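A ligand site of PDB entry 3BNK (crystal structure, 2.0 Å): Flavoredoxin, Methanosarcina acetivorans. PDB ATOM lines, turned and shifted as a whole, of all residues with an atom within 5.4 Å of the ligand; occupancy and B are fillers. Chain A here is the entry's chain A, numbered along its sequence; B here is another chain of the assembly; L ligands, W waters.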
ATOM      1  N   MET A  16      36.172  17.037 -34.596  1.00  0.00           N
ATOM      2  CA  MET A  16      35.904  16.793 -33.185  1.00  0.00           C
ATOM      3  C   MET A  16      36.324  15.359 -32.840  1.00  0.00           C
ATOM      4  O   MET A  16      36.336  14.484 -33.727  1.00  0.00           O
ATOM      5  CB  MET A  16      34.419  16.973 -32.873  1.00  0.00           C
ATOM      6  CG  MET A  16      33.996  18.431 -32.622  1.00  0.00           C
ATOM      7  SD  MET A  16      32.210  18.687 -32.714  1.00  0.00           S
ATOM      8  CE  MET A  16      31.480  17.370 -31.803  1.00  0.00           C
ATOM      9  N   VAL A  18      35.370  11.719 -31.012  1.00  0.00           N
ATOM     10  CA  VAL A  18      34.124  10.990 -30.863  1.00  0.00           C
ATOM     11  C   VAL A  18      34.175  10.133 -29.609  1.00  0.00           C
ATOM     12  O   VAL A  18      34.965   9.192 -29.474  1.00  0.00           O
ATOM     13  CB  VAL A  18      33.727  10.162 -32.115  1.00  0.00           C
ATOM     14  CG1 VAL A  18      32.509   9.285 -31.809  1.00  0.00           C
ATOM     15  CG2 VAL A  18      33.416  11.082 -33.262  1.00  0.00           C
ATOM     16  N   ASN A  30      23.321   5.777 -18.412  1.00  0.00           N
ATOM     17  CA  ASN A  30      22.946   6.470 -19.625  1.00  0.00           C
ATOM     18  C   ASN A  30      24.198   6.841 -20.365  1.00  0.00           C
ATOM     19  O   ASN A  30      25.209   7.173 -19.745  1.00  0.00           O
ATOM     20  CB  ASN A  30      22.146   7.737 -19.308  1.00  0.00           C
ATOM     21  CG  ASN A  30      21.468   8.315 -20.522  1.00  0.00           C
ATOM     22  OD1 ASN A  30      20.712   7.623 -21.204  1.00  0.00           O
ATOM     23  ND2 ASN A  30      21.732   9.592 -20.808  1.00  0.00           N
ATOM     24  N   LEU A  31      24.114   6.810 -21.699  1.00  0.00           N
ATOM     25  CA  LEU A  31      25.200   7.216 -22.584  1.00  0.00           C
ATOM     26  C   LEU A  31      24.701   8.169 -23.647  1.00  0.00           C
ATOM     27  O   LEU A  31      23.612   8.001 -24.178  1.00  0.00           O
ATOM     28  CB  LEU A  31      25.846   5.979 -23.218  1.00  0.00           C
ATOM     29  CG  LEU A  31      26.238   4.981 -22.120  1.00  0.00           C
ATOM     30  CD1 LEU A  31      25.871   3.540 -22.421  1.00  0.00           C
ATOM     31  CD2 LEU A  31      27.688   5.156 -21.687  1.00  0.00           C
ATOM     32  N   MET A  32      25.494   9.201 -23.928  1.00  0.00           N
ATOM     33  CA  MET A  32      25.287  10.070 -25.081  1.00  0.00           C
ATOM     34  C   MET A  32      26.600  10.249 -25.821  1.00  0.00           C
ATOM     35  O   MET A  32      27.685  10.124 -25.235  1.00  0.00           O
ATOM     36  CB  MET A  32      24.698  11.437 -24.697  1.00  0.00           C
ATOM     37  CG  MET A  32      25.512  12.236 -23.673  1.00  0.00           C
ATOM     38  SD  MET A  32      24.962  13.924 -23.552  1.00  0.00           S
ATOM     39  CE  MET A  32      26.058  14.750 -24.695  1.00  0.00           C
ATOM     40  N   ALA A  33      26.479  10.488 -27.123  1.00  0.00           N
ATOM     41  CA  ALA A  33      27.625  10.838 -27.956  1.00  0.00           C
ATOM     42  C   ALA A  33      28.082  12.255 -27.628  1.00  0.00           C
ATOM     43  O   ALA A  33      27.256  13.145 -27.362  1.00  0.00           O
ATOM     44  CB  ALA A  33      27.274  10.696 -29.424  1.00  0.00           C
ATOM     45  N   LEU A  34      29.396  12.452 -27.651  1.00  0.00           N
ATOM     46  CA  LEU A  34      29.991  13.677 -27.178  1.00  0.00           C
ATOM     47  C   LEU A  34      31.246  14.057 -27.953  1.00  0.00           C
ATOM     48  O   LEU A  34      32.249  13.353 -27.905  1.00  0.00           O
ATOM     49  CB  LEU A  34      30.304  13.559 -25.676  1.00  0.00           C
ATOM     50  CG  LEU A  34      30.992  14.715 -24.963  1.00  0.00           C
ATOM     51  CD1 LEU A  34      29.975  15.772 -24.506  1.00  0.00           C
ATOM     52  CD2 LEU A  34      31.808  14.183 -23.754  1.00  0.00           C
ATOM     53  N   GLY A  35      31.200  15.194 -28.641  1.00  0.00           N
ATOM     54  CA  GLY A  35      32.386  15.756 -29.303  1.00  0.00           C
ATOM     55  C   GLY A  35      32.971  16.989 -28.615  1.00  0.00           C
ATOM     56  O   GLY A  35      34.059  17.456 -28.963  1.00  0.00           O
ATOM     57  N   TRP A  36      32.243  17.514 -27.643  1.00  0.00           N
ATOM     58  CA  TRP A  36      32.660  18.728 -26.950  1.00  0.00           C
ATOM     59  C   TRP A  36      33.370  18.358 -25.649  1.00  0.00           C
ATOM     60  O   TRP A  36      32.811  18.489 -24.547  1.00  0.00           O
ATOM     61  CB  TRP A  36      31.449  19.619 -26.673  1.00  0.00           C
ATOM     62  CG  TRP A  36      30.788  20.207 -27.925  1.00  0.00           C
ATOM     63  CD1 TRP A  36      30.947  19.794 -29.236  1.00  0.00           C
ATOM     64  CD2 TRP A  36      29.832  21.264 -27.967  1.00  0.00           C
ATOM     65  NE1 TRP A  36      30.166  20.548 -30.073  1.00  0.00           N
ATOM     66  CE2 TRP A  36      29.468  21.467 -29.317  1.00  0.00           C
ATOM     67  CE3 TRP A  36      29.243  22.082 -26.981  1.00  0.00           C
ATOM     68  CZ2 TRP A  36      28.541  22.459 -29.724  1.00  0.00           C
ATOM     69  CZ3 TRP A  36      28.338  23.069 -27.388  1.00  0.00           C
ATOM     70  CH2 TRP A  36      27.990  23.236 -28.755  1.00  0.00           C
ATOM     71  N   GLY A  50      31.112  19.538 -22.610  1.00  0.00           N
ATOM     72  CA  GLY A  50      30.056  20.481 -23.001  1.00  0.00           C
ATOM     73  C   GLY A  50      28.726  19.824 -23.373  1.00  0.00           C
ATOM     74  O   GLY A  50      28.603  19.170 -24.430  1.00  0.00           O
ATOM     75  N   VAL A  51      27.731  20.021 -22.523  1.00  0.00           N
ATOM     76  CA  VAL A  51      26.508  19.219 -22.583  1.00  0.00           C
ATOM     77  C   VAL A  51      25.255  20.077 -22.647  1.00  0.00           C
ATOM     78  O   VAL A  51      25.023  20.927 -21.770  1.00  0.00           O
ATOM     79  CB  VAL A  51      26.393  18.286 -21.353  1.00  0.00           C
ATOM     80  CG1 VAL A  51      25.218  17.302 -21.536  1.00  0.00           C
ATOM     81  CG2 VAL A  51      27.680  17.521 -21.145  1.00  0.00           C
ATOM     82  N   ASN A  52      24.443  19.871 -23.686  1.00  0.00           N
ATOM     83  CA  ASN A  52      23.214  20.637 -23.811  1.00  0.00           C
ATOM     84  C   ASN A  52      22.247  20.468 -22.640  1.00  0.00           C
ATOM     85  O   ASN A  52      21.986  19.364 -22.154  1.00  0.00           O
ATOM     86  CB  ASN A  52      22.530  20.428 -25.170  1.00  0.00           C
ATOM     87  CG  ASN A  52      21.671  21.631 -25.569  1.00  0.00           C
ATOM     88  OD1 ASN A  52      20.597  21.846 -25.013  1.00  0.00           O
ATOM     89  ND2 ASN A  52      22.159  22.427 -26.515  1.00  0.00           N
ATOM     90  N   SER A  54      19.219  20.618 -22.772  1.00  0.00           N
ATOM     91  CA  SER A  54      18.034  19.889 -23.275  1.00  0.00           C
ATOM     92  C   SER A  54      18.179  18.371 -23.205  1.00  0.00           C
ATOM     93  O   SER A  54      17.233  17.636 -23.513  1.00  0.00           O
ATOM     94  CB  SER A  54      17.676  20.328 -24.709  1.00  0.00           C
ATOM     95  OG  SER A  54      18.460  19.653 -25.689  1.00  0.00           O
ATOM     96  N   HIS A  55      19.352  17.903 -22.776  1.00  0.00           N
ATOM     97  CA  HIS A  55      19.644  16.475 -22.719  1.00  0.00           C
ATOM     98  C   HIS A  55      19.318  15.882 -21.356  1.00  0.00           C
ATOM     99  O   HIS A  55      19.164  16.617 -20.371  1.00  0.00           O
ATOM    100  CB  HIS A  55      21.108  16.164 -23.084  1.00  0.00           C
ATOM    101  CG  HIS A  55      21.486  16.539 -24.490  1.00  0.00           C
ATOM    102  ND1 HIS A  55      20.558  16.699 -25.499  1.00  0.00           N
ATOM    103  CD2 HIS A  55      22.689  16.768 -25.050  1.00  0.00           C
ATOM    104  CE1 HIS A  55      21.180  17.039 -26.612  1.00  0.00           C
ATOM    105  NE2 HIS A  55      22.475  17.077 -26.375  1.00  0.00           N
ATOM    106  N   TYR A  56      19.229  14.552 -21.318  1.00  0.00           N
ATOM    107  CA  TYR A  56      18.909  13.788 -20.135  1.00  0.00           C
ATOM    108  C   TYR A  56      20.138  13.540 -19.269  1.00  0.00           C
ATOM    109  O   TYR A  56      20.035  13.405 -18.041  1.00  0.00           O
ATOM    110  CB  TYR A  56      18.300  12.443 -20.559  1.00  0.00           C
ATOM    111  CG  TYR A  56      17.701  11.602 -19.459  1.00  0.00           C
ATOM    112  CD1 TYR A  56      16.596  12.039 -18.722  1.00  0.00           C
ATOM    113  CD2 TYR A  56      18.198  10.330 -19.195  1.00  0.00           C
ATOM    114  CE1 TYR A  56      16.039  11.256 -17.723  1.00  0.00           C
ATOM    115  CE2 TYR A  56      17.649   9.536 -18.203  1.00  0.00           C
ATOM    116  CZ  TYR A  56      16.563   9.999 -17.467  1.00  0.00           C
ATOM    117  OH  TYR A  56      16.005   9.204 -16.496  1.00  0.00           O
ATOM    118  N   THR A  57      21.303  13.488 -19.907  1.00  0.00           N
ATOM    119  CA  THR A  57      22.558  13.165 -19.217  1.00  0.00           C
ATOM    120  C   THR A  57      22.949  14.126 -18.052  1.00  0.00           C
ATOM    121  O   THR A  57      23.368  13.642 -17.002  1.00  0.00           O
ATOM    122  CB  THR A  57      23.730  12.981 -20.224  1.00  0.00           C
ATOM    123  OG1 THR A  57      23.431  11.870 -21.084  1.00  0.00           O
ATOM    124  CG2 THR A  57      25.046  12.712 -19.516  1.00  0.00           C
ATOM    125  N   PRO A  58      22.795  15.475 -18.236  1.00  0.00           N
ATOM    126  CA  PRO A  58      23.177  16.425 -17.174  1.00  0.00           C
ATOM    127  C   PRO A  58      22.465  16.213 -15.827  1.00  0.00           C
ATOM    128  O   PRO A  58      23.067  16.466 -14.774  1.00  0.00           O
ATOM    129  CB  PRO A  58      22.786  17.786 -17.750  1.00  0.00           C
ATOM    130  CG  PRO A  58      22.639  17.592 -19.220  1.00  0.00           C
ATOM    131  CD  PRO A  58      22.272  16.162 -19.438  1.00  0.00           C
ATOM    132  N   THR A  80      27.145   4.049 -31.597  1.00  0.00           N
ATOM    133  CA  THR A  80      27.642   5.363 -31.175  1.00  0.00           C
ATOM    134  C   THR A  80      26.743   6.498 -31.675  1.00  0.00           C
ATOM    135  O   THR A  80      26.365   7.378 -30.888  1.00  0.00           O
ATOM    136  CB  THR A  80      29.106   5.585 -31.628  1.00  0.00           C
ATOM    137  OG1 THR A  80      29.928   4.556 -31.070  1.00  0.00           O
ATOM    138  CG2 THR A  80      29.635   6.949 -31.186  1.00  0.00           C
ATOM    139  N   ASP A  81      26.421   6.473 -32.955  1.00  0.00           N
ATOM    140  CA  ASP A  81      25.505   7.472 -33.539  1.00  0.00           C
ATOM    141  C   ASP A  81      24.093   7.365 -32.952  1.00  0.00           C
ATOM    142  O   ASP A  81      23.445   8.382 -32.714  1.00  0.00           O
ATOM    143  CB  ASP A  81      25.451   7.320 -35.052  1.00  0.00           C
ATOM    144  CG  ASP A  81      25.013   8.590 -35.762  1.00  0.00           C
ATOM    145  OD1 ASP A  81      25.607   9.668 -35.520  1.00  0.00           O
ATOM    146  OD2 ASP A  81      24.090   8.493 -36.590  1.00  0.00           O
ATOM    147  N   TYR A  82      23.626   6.129 -32.747  1.00  0.00           N
ATOM    148  CA  TYR A  82      22.369   5.864 -32.029  1.00  0.00           C
ATOM    149  C   TYR A  82      22.296   6.604 -30.694  1.00  0.00           C
ATOM    150  O   TYR A  82      21.320   7.284 -30.409  1.00  0.00           O
ATOM    151  CB  TYR A  82      22.190   4.372 -31.811  1.00  0.00           C
ATOM    152  CG  TYR A  82      20.863   3.999 -31.186  1.00  0.00           C
ATOM    153  CD1 TYR A  82      19.674   4.224 -31.872  1.00  0.00           C
ATOM    154  CD2 TYR A  82      20.797   3.438 -29.905  1.00  0.00           C
ATOM    155  CE1 TYR A  82      18.450   3.899 -31.315  1.00  0.00           C
ATOM    156  CE2 TYR A  82      19.568   3.113 -29.327  1.00  0.00           C
ATOM    157  CZ  TYR A  82      18.396   3.348 -30.050  1.00  0.00           C
ATOM    158  OH  TYR A  82      17.162   3.034 -29.519  1.00  0.00           O
ATOM    159  N   CYS A  83      23.360   6.473 -29.888  1.00  0.00           N
ATOM    160  CA  CYS A  83      23.503   7.207 -28.617  1.00  0.00           C
ATOM    161  C   CYS A  83      23.523   8.718 -28.758  1.00  0.00           C
ATOM    162  O   CYS A  83      23.239   9.443 -27.794  1.00  0.00           O
ATOM    163  CB  CYS A  83      24.747   6.731 -27.886  1.00  0.00           C
ATOM    164  SG  CYS A  83      24.528   5.108 -27.234  1.00  0.00           S
ATOM    165  N   GLY A  84      23.854   9.208 -29.938  1.00  0.00           N
ATOM    166  CA  GLY A  84      23.761  10.632 -30.242  1.00  0.00           C
ATOM    167  C   GLY A  84      22.445  11.069 -30.856  1.00  0.00           C
ATOM    168  O   GLY A  84      22.323  12.213 -31.272  1.00  0.00           O
ATOM    169  N   LEU A  85      21.469  10.178 -30.948  1.00  0.00           N
ATOM    170  CA  LEU A  85      20.187  10.506 -31.616  1.00  0.00           C
ATOM    171  C   LEU A  85      19.007  10.338 -30.661  1.00  0.00           C
ATOM    172  O   LEU A  85      18.056  11.139 -30.675  1.00  0.00           O
ATOM    173  CB  LEU A  85      19.991   9.610 -32.851  1.00  0.00           C
ATOM    174  CG  LEU A  85      20.676  10.006 -34.153  1.00  0.00           C
ATOM    175  CD1 LEU A  85      20.930   8.762 -35.022  1.00  0.00           C
ATOM    176  CD2 LEU A  85      19.836  11.032 -34.903  1.00  0.00           C
ATOM    177  N   VAL A  86      19.070   9.298 -29.851  1.00  0.00           N
ATOM    178  CA  VAL A  86      18.002   8.961 -28.931  1.00  0.00           C
ATOM    179  C   VAL A  86      18.361   9.504 -27.517  1.00  0.00           C
ATOM    180  O   VAL A  86      19.531   9.556 -27.149  1.00  0.00           O
ATOM    181  CB  VAL A  86      17.802   7.419 -28.983  1.00  0.00           C
ATOM    182  CG1 VAL A  86      17.365   6.873 -27.698  1.00  0.00           C
ATOM    183  CG2 VAL A  86      16.833   7.033 -30.135  1.00  0.00           C
ATOM    184  N   SER A  87      17.357   9.949 -26.756  1.00  0.00           N
ATOM    185  CA  SER A  87      17.577  10.413 -25.379  1.00  0.00           C
ATOM    186  C   SER A  87      17.131   9.376 -24.359  1.00  0.00           C
ATOM    187  O   SER A  87      16.111   8.715 -24.552  1.00  0.00           O
ATOM    188  CB  SER A  87      16.834  11.728 -25.095  1.00  0.00           C
ATOM    189  OG  SER A  87      16.956  12.092 -23.726  1.00  0.00           O
ATOM    190  N   GLY A  88      17.905   9.254 -23.282  1.00  0.00           N
ATOM    191  CA  GLY A  88      17.575   8.373 -22.159  1.00  0.00           C
ATOM    192  C   GLY A  88      16.271   8.745 -21.481  1.00  0.00           C
ATOM    193  O   GLY A  88      15.737   7.972 -20.694  1.00  0.00           O
ATOM    194  N   GLU A  89      15.763   9.938 -21.788  1.00  0.00           N
ATOM    195  CA  GLU A  89      14.436  10.390 -21.347  1.00  0.00           C
ATOM    196  C   GLU A  89      13.339   9.429 -21.825  1.00  0.00           C
ATOM    197  O   GLU A  89      12.445   9.073 -21.047  1.00  0.00           O
ATOM    198  CB  GLU A  89      14.174  11.833 -21.834  1.00  0.00           C
ATOM    199  CG  GLU A  89      12.822  12.441 -21.434  1.00  0.00           C
ATOM    200  CD  GLU A  89      12.484  13.722 -22.208  1.00  0.00           C
ATOM    201  OE1 GLU A  89      13.404  14.441 -22.660  1.00  0.00           O
ATOM    202  OE2 GLU A  89      11.273  14.027 -22.362  1.00  0.00           O
ATOM    203  N   LYS A  93      19.068   3.300 -22.585  1.00  0.00           N
ATOM    204  CA  LYS A  93      20.310   2.975 -23.278  1.00  0.00           C
ATOM    205  C   LYS A  93      21.271   2.149 -22.411  1.00  0.00           C
ATOM    206  O   LYS A  93      22.391   1.870 -22.835  1.00  0.00           O
ATOM    207  CB  LYS A  93      20.994   4.263 -23.787  1.00  0.00           C
ATOM    208  CG  LYS A  93      20.394   4.852 -25.075  1.00  0.00           C
ATOM    209  CD  LYS A  93      21.036   6.178 -25.456  1.00  0.00           C
ATOM    210  CE  LYS A  93      20.408   7.344 -24.696  1.00  0.00           C
ATOM    211  NZ  LYS A  93      21.067   8.652 -24.995  1.00  0.00           N
ATOM    212  N   ASN A 130      24.182  25.264 -22.430  1.00  0.00           N
ATOM    213  CA  ASN A 130      24.974  24.099 -22.108  1.00  0.00           C
ATOM    214  C   ASN A 130      25.570  24.197 -20.732  1.00  0.00           C
ATOM    215  O   ASN A 130      26.043  25.266 -20.339  1.00  0.00           O
ATOM    216  CB  ASN A 130      26.166  23.980 -23.055  1.00  0.00           C
ATOM    217  CG  ASN A 130      25.777  23.745 -24.494  1.00  0.00           C
ATOM    218  OD1 ASN A 130      25.282  24.643 -25.179  1.00  0.00           O
ATOM    219  ND2 ASN A 130      26.055  22.539 -24.991  1.00  0.00           N
ATOM    220  N   LEU A 162      34.832  13.464 -35.965  1.00  0.00           N
ATOM    221  CA  LEU A 162      33.543  13.997 -36.348  1.00  0.00           C
ATOM    222  C   LEU A 162      33.634  15.418 -36.889  1.00  0.00           C
ATOM    223  O   LEU A 162      34.333  16.273 -36.357  1.00  0.00           O
ATOM    224  CB  LEU A 162      32.507  13.938 -35.186  1.00  0.00           C
ATOM    225  CG  LEU A 162      31.180  14.706 -35.372  1.00  0.00           C
ATOM    226  CD1 LEU A 162      30.203  13.892 -36.251  1.00  0.00           C
ATOM    227  CD2 LEU A 162      30.519  15.061 -34.063  1.00  0.00           C
ATOM    228  N   MET A 164      30.838  18.552 -38.130  1.00  0.00           N
ATOM    229  CA  MET A 164      29.471  19.086 -38.197  1.00  0.00           C
ATOM    230  C   MET A 164      29.512  20.526 -38.732  1.00  0.00           C
ATOM    231  O   MET A 164      30.548  21.190 -38.594  1.00  0.00           O
ATOM    232  CB  MET A 164      28.838  19.082 -36.798  1.00  0.00           C
ATOM    233  CG  MET A 164      28.441  17.708 -36.270  1.00  0.00           C
ATOM    234  SD  MET A 164      27.604  17.786 -34.677  1.00  0.00           S
ATOM    235  CE  MET A 164      26.850  16.150 -34.575  1.00  0.00           C
ATOM    236  N   TYR A 169      31.501  11.224 -40.112  1.00  0.00           N
ATOM    237  CA  TYR A 169      32.508  10.492 -39.350  1.00  0.00           C
ATOM    238  C   TYR A 169      33.737  10.292 -40.223  1.00  0.00           C
ATOM    239  O   TYR A 169      33.625  10.193 -41.452  1.00  0.00           O
ATOM    240  CB  TYR A 169      31.973   9.127 -38.851  1.00  0.00           C
ATOM    241  CG  TYR A 169      30.955   9.230 -37.734  1.00  0.00           C
ATOM    242  CD1 TYR A 169      29.638   8.789 -37.914  1.00  0.00           C
ATOM    243  CD2 TYR A 169      31.302   9.797 -36.503  1.00  0.00           C
ATOM    244  CE1 TYR A 169      28.705   8.872 -36.891  1.00  0.00           C
ATOM    245  CE2 TYR A 169      30.374   9.904 -35.479  1.00  0.00           C
ATOM    246  CZ  TYR A 169      29.072   9.445 -35.674  1.00  0.00           C
ATOM    247  OH  TYR A 169      28.164   9.560 -34.655  1.00  0.00           O
ATOM    248  N   ALA B 179      27.047  10.933 -39.682  1.00  0.00           N
ATOM    249  CA  ALA B 179      26.674  11.271 -38.297  1.00  0.00           C
ATOM    250  C   ALA B 179      25.241  11.794 -38.236  1.00  0.00           C
ATOM    251  O   ALA B 179      24.789  12.416 -39.200  1.00  0.00           O
ATOM    252  CB  ALA B 179      27.630  12.292 -37.738  1.00  0.00           C
ATOM    253  N   LEU B 180      24.539  11.550 -37.125  1.00  0.00           N
ATOM    254  CA  LEU B 180      23.120  11.910 -36.999  1.00  0.00           C
ATOM    255  C   LEU B 180      22.313  11.298 -38.154  1.00  0.00           C
ATOM    256  O   LEU B 180      21.461  11.960 -38.776  1.00  0.00           O
ATOM    257  CB  LEU B 180      22.942  13.440 -36.953  1.00  0.00           C
ATOM    258  CG  LEU B 180      23.511  14.209 -35.751  1.00  0.00           C
ATOM    259  CD1 LEU B 180      23.377  15.695 -35.960  1.00  0.00           C
ATOM    260  CD2 LEU B 180      22.797  13.786 -34.469  1.00  0.00           C
HETATM  261  N1  LIG L   1      25.455  16.939 -27.445  1.00  0.00           N
HETATM  262  C1  LIG L   1      26.083  17.755 -26.547  1.00  0.00           C
HETATM  263  O1  LIG L   1      25.383  18.347 -25.744  1.00  0.00           O
HETATM  264  N2  LIG L   1      27.471  17.891 -26.593  1.00  0.00           N
HETATM  265  C2  LIG L   1      28.213  17.174 -27.531  1.00  0.00           C
HETATM  266  O2  LIG L   1      29.433  17.232 -27.546  1.00  0.00           O
HETATM  267  C3  LIG L   1      27.557  16.335 -28.439  1.00  0.00           C
HETATM  268  N3  LIG L   1      28.275  15.635 -29.383  1.00  0.00           N
HETATM  269  C4  LIG L   1      27.627  14.793 -30.281  1.00  0.00           C
HETATM  270  C5  LIG L   1      28.382  14.094 -31.216  1.00  0.00           C
HETATM  271  C6  LIG L   1      27.749  13.234 -32.128  1.00  0.00           C
HETATM  272  C7  LIG L   1      28.593  12.194 -32.811  1.00  0.00           C
HETATM  273  C8  LIG L   1      26.353  13.103 -32.084  1.00  0.00           C
HETATM  274  C9  LIG L   1      25.635  12.070 -32.921  1.00  0.00           C
HETATM  275  C10 LIG L   1      25.603  13.823 -31.157  1.00  0.00           C
HETATM  276  C11 LIG L   1      26.224  14.669 -30.239  1.00  0.00           C
HETATM  277  N4  LIG L   1      25.497  15.395 -29.284  1.00  0.00           N
HETATM  278  C12 LIG L   1      26.160  16.221 -28.392  1.00  0.00           C
HETATM  279  C13 LIG L   1      23.998  15.249 -29.131  1.00  0.00           C
HETATM  280  C14 LIG L   1      23.658  14.197 -28.067  1.00  0.00           C
HETATM  281  O3  LIG L   1      24.616  13.156 -28.139  1.00  0.00           O
HETATM  282  C15 LIG L   1      22.262  13.633 -28.301  1.00  0.00           C
HETATM  283  O4  LIG L   1      21.293  14.665 -28.268  1.00  0.00           O
HETATM  284  C16 LIG L   1      21.832  12.511 -27.344  1.00  0.00           C
HETATM  285  O5  LIG L   1      20.665  11.930 -27.886  1.00  0.00           O
HETATM  286  C17 LIG L   1      21.568  13.005 -25.931  1.00  0.00           C
HETATM  287  O6  LIG L   1      21.029  11.941 -25.176  1.00  0.00           O
HETATM  288  P1  LIG L   1      20.544  12.077 -23.647  1.00  0.00           P
HETATM  289  O7  LIG L   1      19.323  12.957 -23.722  1.00  0.00           O
HETATM  290  O8  LIG L   1      21.573  12.769 -22.786  1.00  0.00           O
HETATM  291  O9  LIG L   1      20.270  10.674 -23.136  1.00  0.00           O
HETATM  292  O   HOH W   1      20.718  14.402 -31.135  1.00  0.00           O
HETATM  293  O   HOH W   2      18.309  15.882 -28.891  1.00  0.00           O
HETATM  294  O   HOH W   3      18.315  13.484 -27.947  1.00  0.00           O
HETATM  295  O   HOH W   4      23.013  18.906 -28.858  1.00  0.00           O
HETATM  296  O   HOH W   5      18.404  14.739 -25.511  1.00  0.00           O
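The side-chain amino group (NZ) of Lys 93 lies within hydrogen-bond range of the backbone carbonyl oxygen (O) of Val 86 (2.8 Å). OD1 of Asp 81 lies within hydrogen-bond range of N of Leu 180 of chain B (2.7 Å). The backbone NH of Ser 54 is in hydrogen-bond range of the side-chain amide oxygen of Asn 52 (2.9 Å). OG of Ser 87 sits close to N of Glu 89 (3.1 Å). The side-chain hydroxyl (OH) of Tyr 169 is in hydrogen-bond range of the side-chain carboxylate (OD1) of Asp 81, 2.7 Å away. O of Leu 162 sits at hydrogen-bond distance from N of Met 16, 2.7 Å away. The side-chain sulfur of Met 32 sits close to the side-chain hydroxyl of Thr 57 (3.6 Å). The backbone NH of Ala 33 sits at hydrogen-bond distance from the backbone carbonyl oxygen of Cys 83.
Water W5 bridges an oxygen (O7) of the ligand and a ring nitrogen (ND1) of His 55. Water W1 lies within hydrogen-bond range of O of Gly 84 (2.7 Å) and O4 of the ligand (2.9 Å). Water W4 bridges NE2 of His 55 and N1 of the ligand.
The backbone NH (N) of Gly 35 is in hydrogen-bond range of an oxygen (O2) of the ligand, at 2.9 Å. O of Gly 50 sits at hydrogen-bond distance from N2 of the ligand (2.8 Å). O7 of the ligand lies within hydrogen-bond range of OG of Ser 87 (2.5 Å). O3 of the ligand is in hydrogen-bond range of N of Ala 33, at 3.4 Å. An oxygen (O2) of the ligand sits at hydrogen-bond distance from the backbone NH (N) of Trp 36, at 2.8 Å. The backbone NH of Asn 52 lies within hydrogen-bond range of an oxygen (O1) of the ligand (2.7 Å). N of Thr 57 lies within hydrogen-bond range of O8 of the ligand, 3.0 Å away. A ring nitrogen (NE2) of His 55 is in hydrogen-bond range of a nitrogen (N1) of the ligand, 3.2 Å away. The backbone carbonyl oxygen of Ala 33 lies within hydrogen-bond range of an oxygen (O3) of the ligand (2.8 Å). OG1 of Thr 57 lies within hydrogen-bond range of O8 of the ligand, 2.7 Å away. An oxygen (O5) of the ligand lies within hydrogen-bond range of the backbone carbonyl oxygen of Val 86 (2.7 Å). NZ of Lys 93 is in salt-bridge range of O9 of the ligand, 2.9 Å away. The backbone NH (N) of Tyr 56 lies within hydrogen-bond range of an oxygen (O7) of the ligand. ND2 of Asn 30 is in hydrogen-bond range of O9 of the ligand. O9 of the ligand lies within hydrogen-bond range of N of Gly 88.
The side-chain sulfur (SD) of Met 32 sits close to an oxygen (O8) of the ligand, 3.7 Å away. Leu 34 touches the ligand (CA to N3, 3.4 Å). Val 51 touches the ligand. Asp 81 touches the ligand (OD1 to C9, 3.5 Å). O of Cys 83 touches C16 of the ligand, 3.4 Å away. Gly 84 touches the ligand (O to C15, 3.3 Å). Leu 85 touches the ligand. Leu 162 touches the ligand. Met 164 touches the ligand (CE to C6, 3.9 Å). Tyr 169 touches the ligand. Leu 180 of chain B touches the ligand (CD2 to C9, 3.7 Å). Hydrophobic or aromatic side chains that line the ligand: Met 32, Ala 33, Leu 34, Trp 36, His 55, Tyr 56, Leu 162, Met 164, Tyr 169 and Leu 180 of chain B. 24 residues have an atom within 4 Å of the ligand: Asn 30, Met 32, Ala 33, Leu 34, Gly 35, Trp 36, Gly 50, Val 51, Asn 52, His 55, Tyr 56, Thr 57, Asp 81, Cys 83, Gly 84, Leu 85, Val 86, Ser 87, Gly 88, Lys 93, Leu 162, Met 164, Tyr 169 and Leu 180 of chain B.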
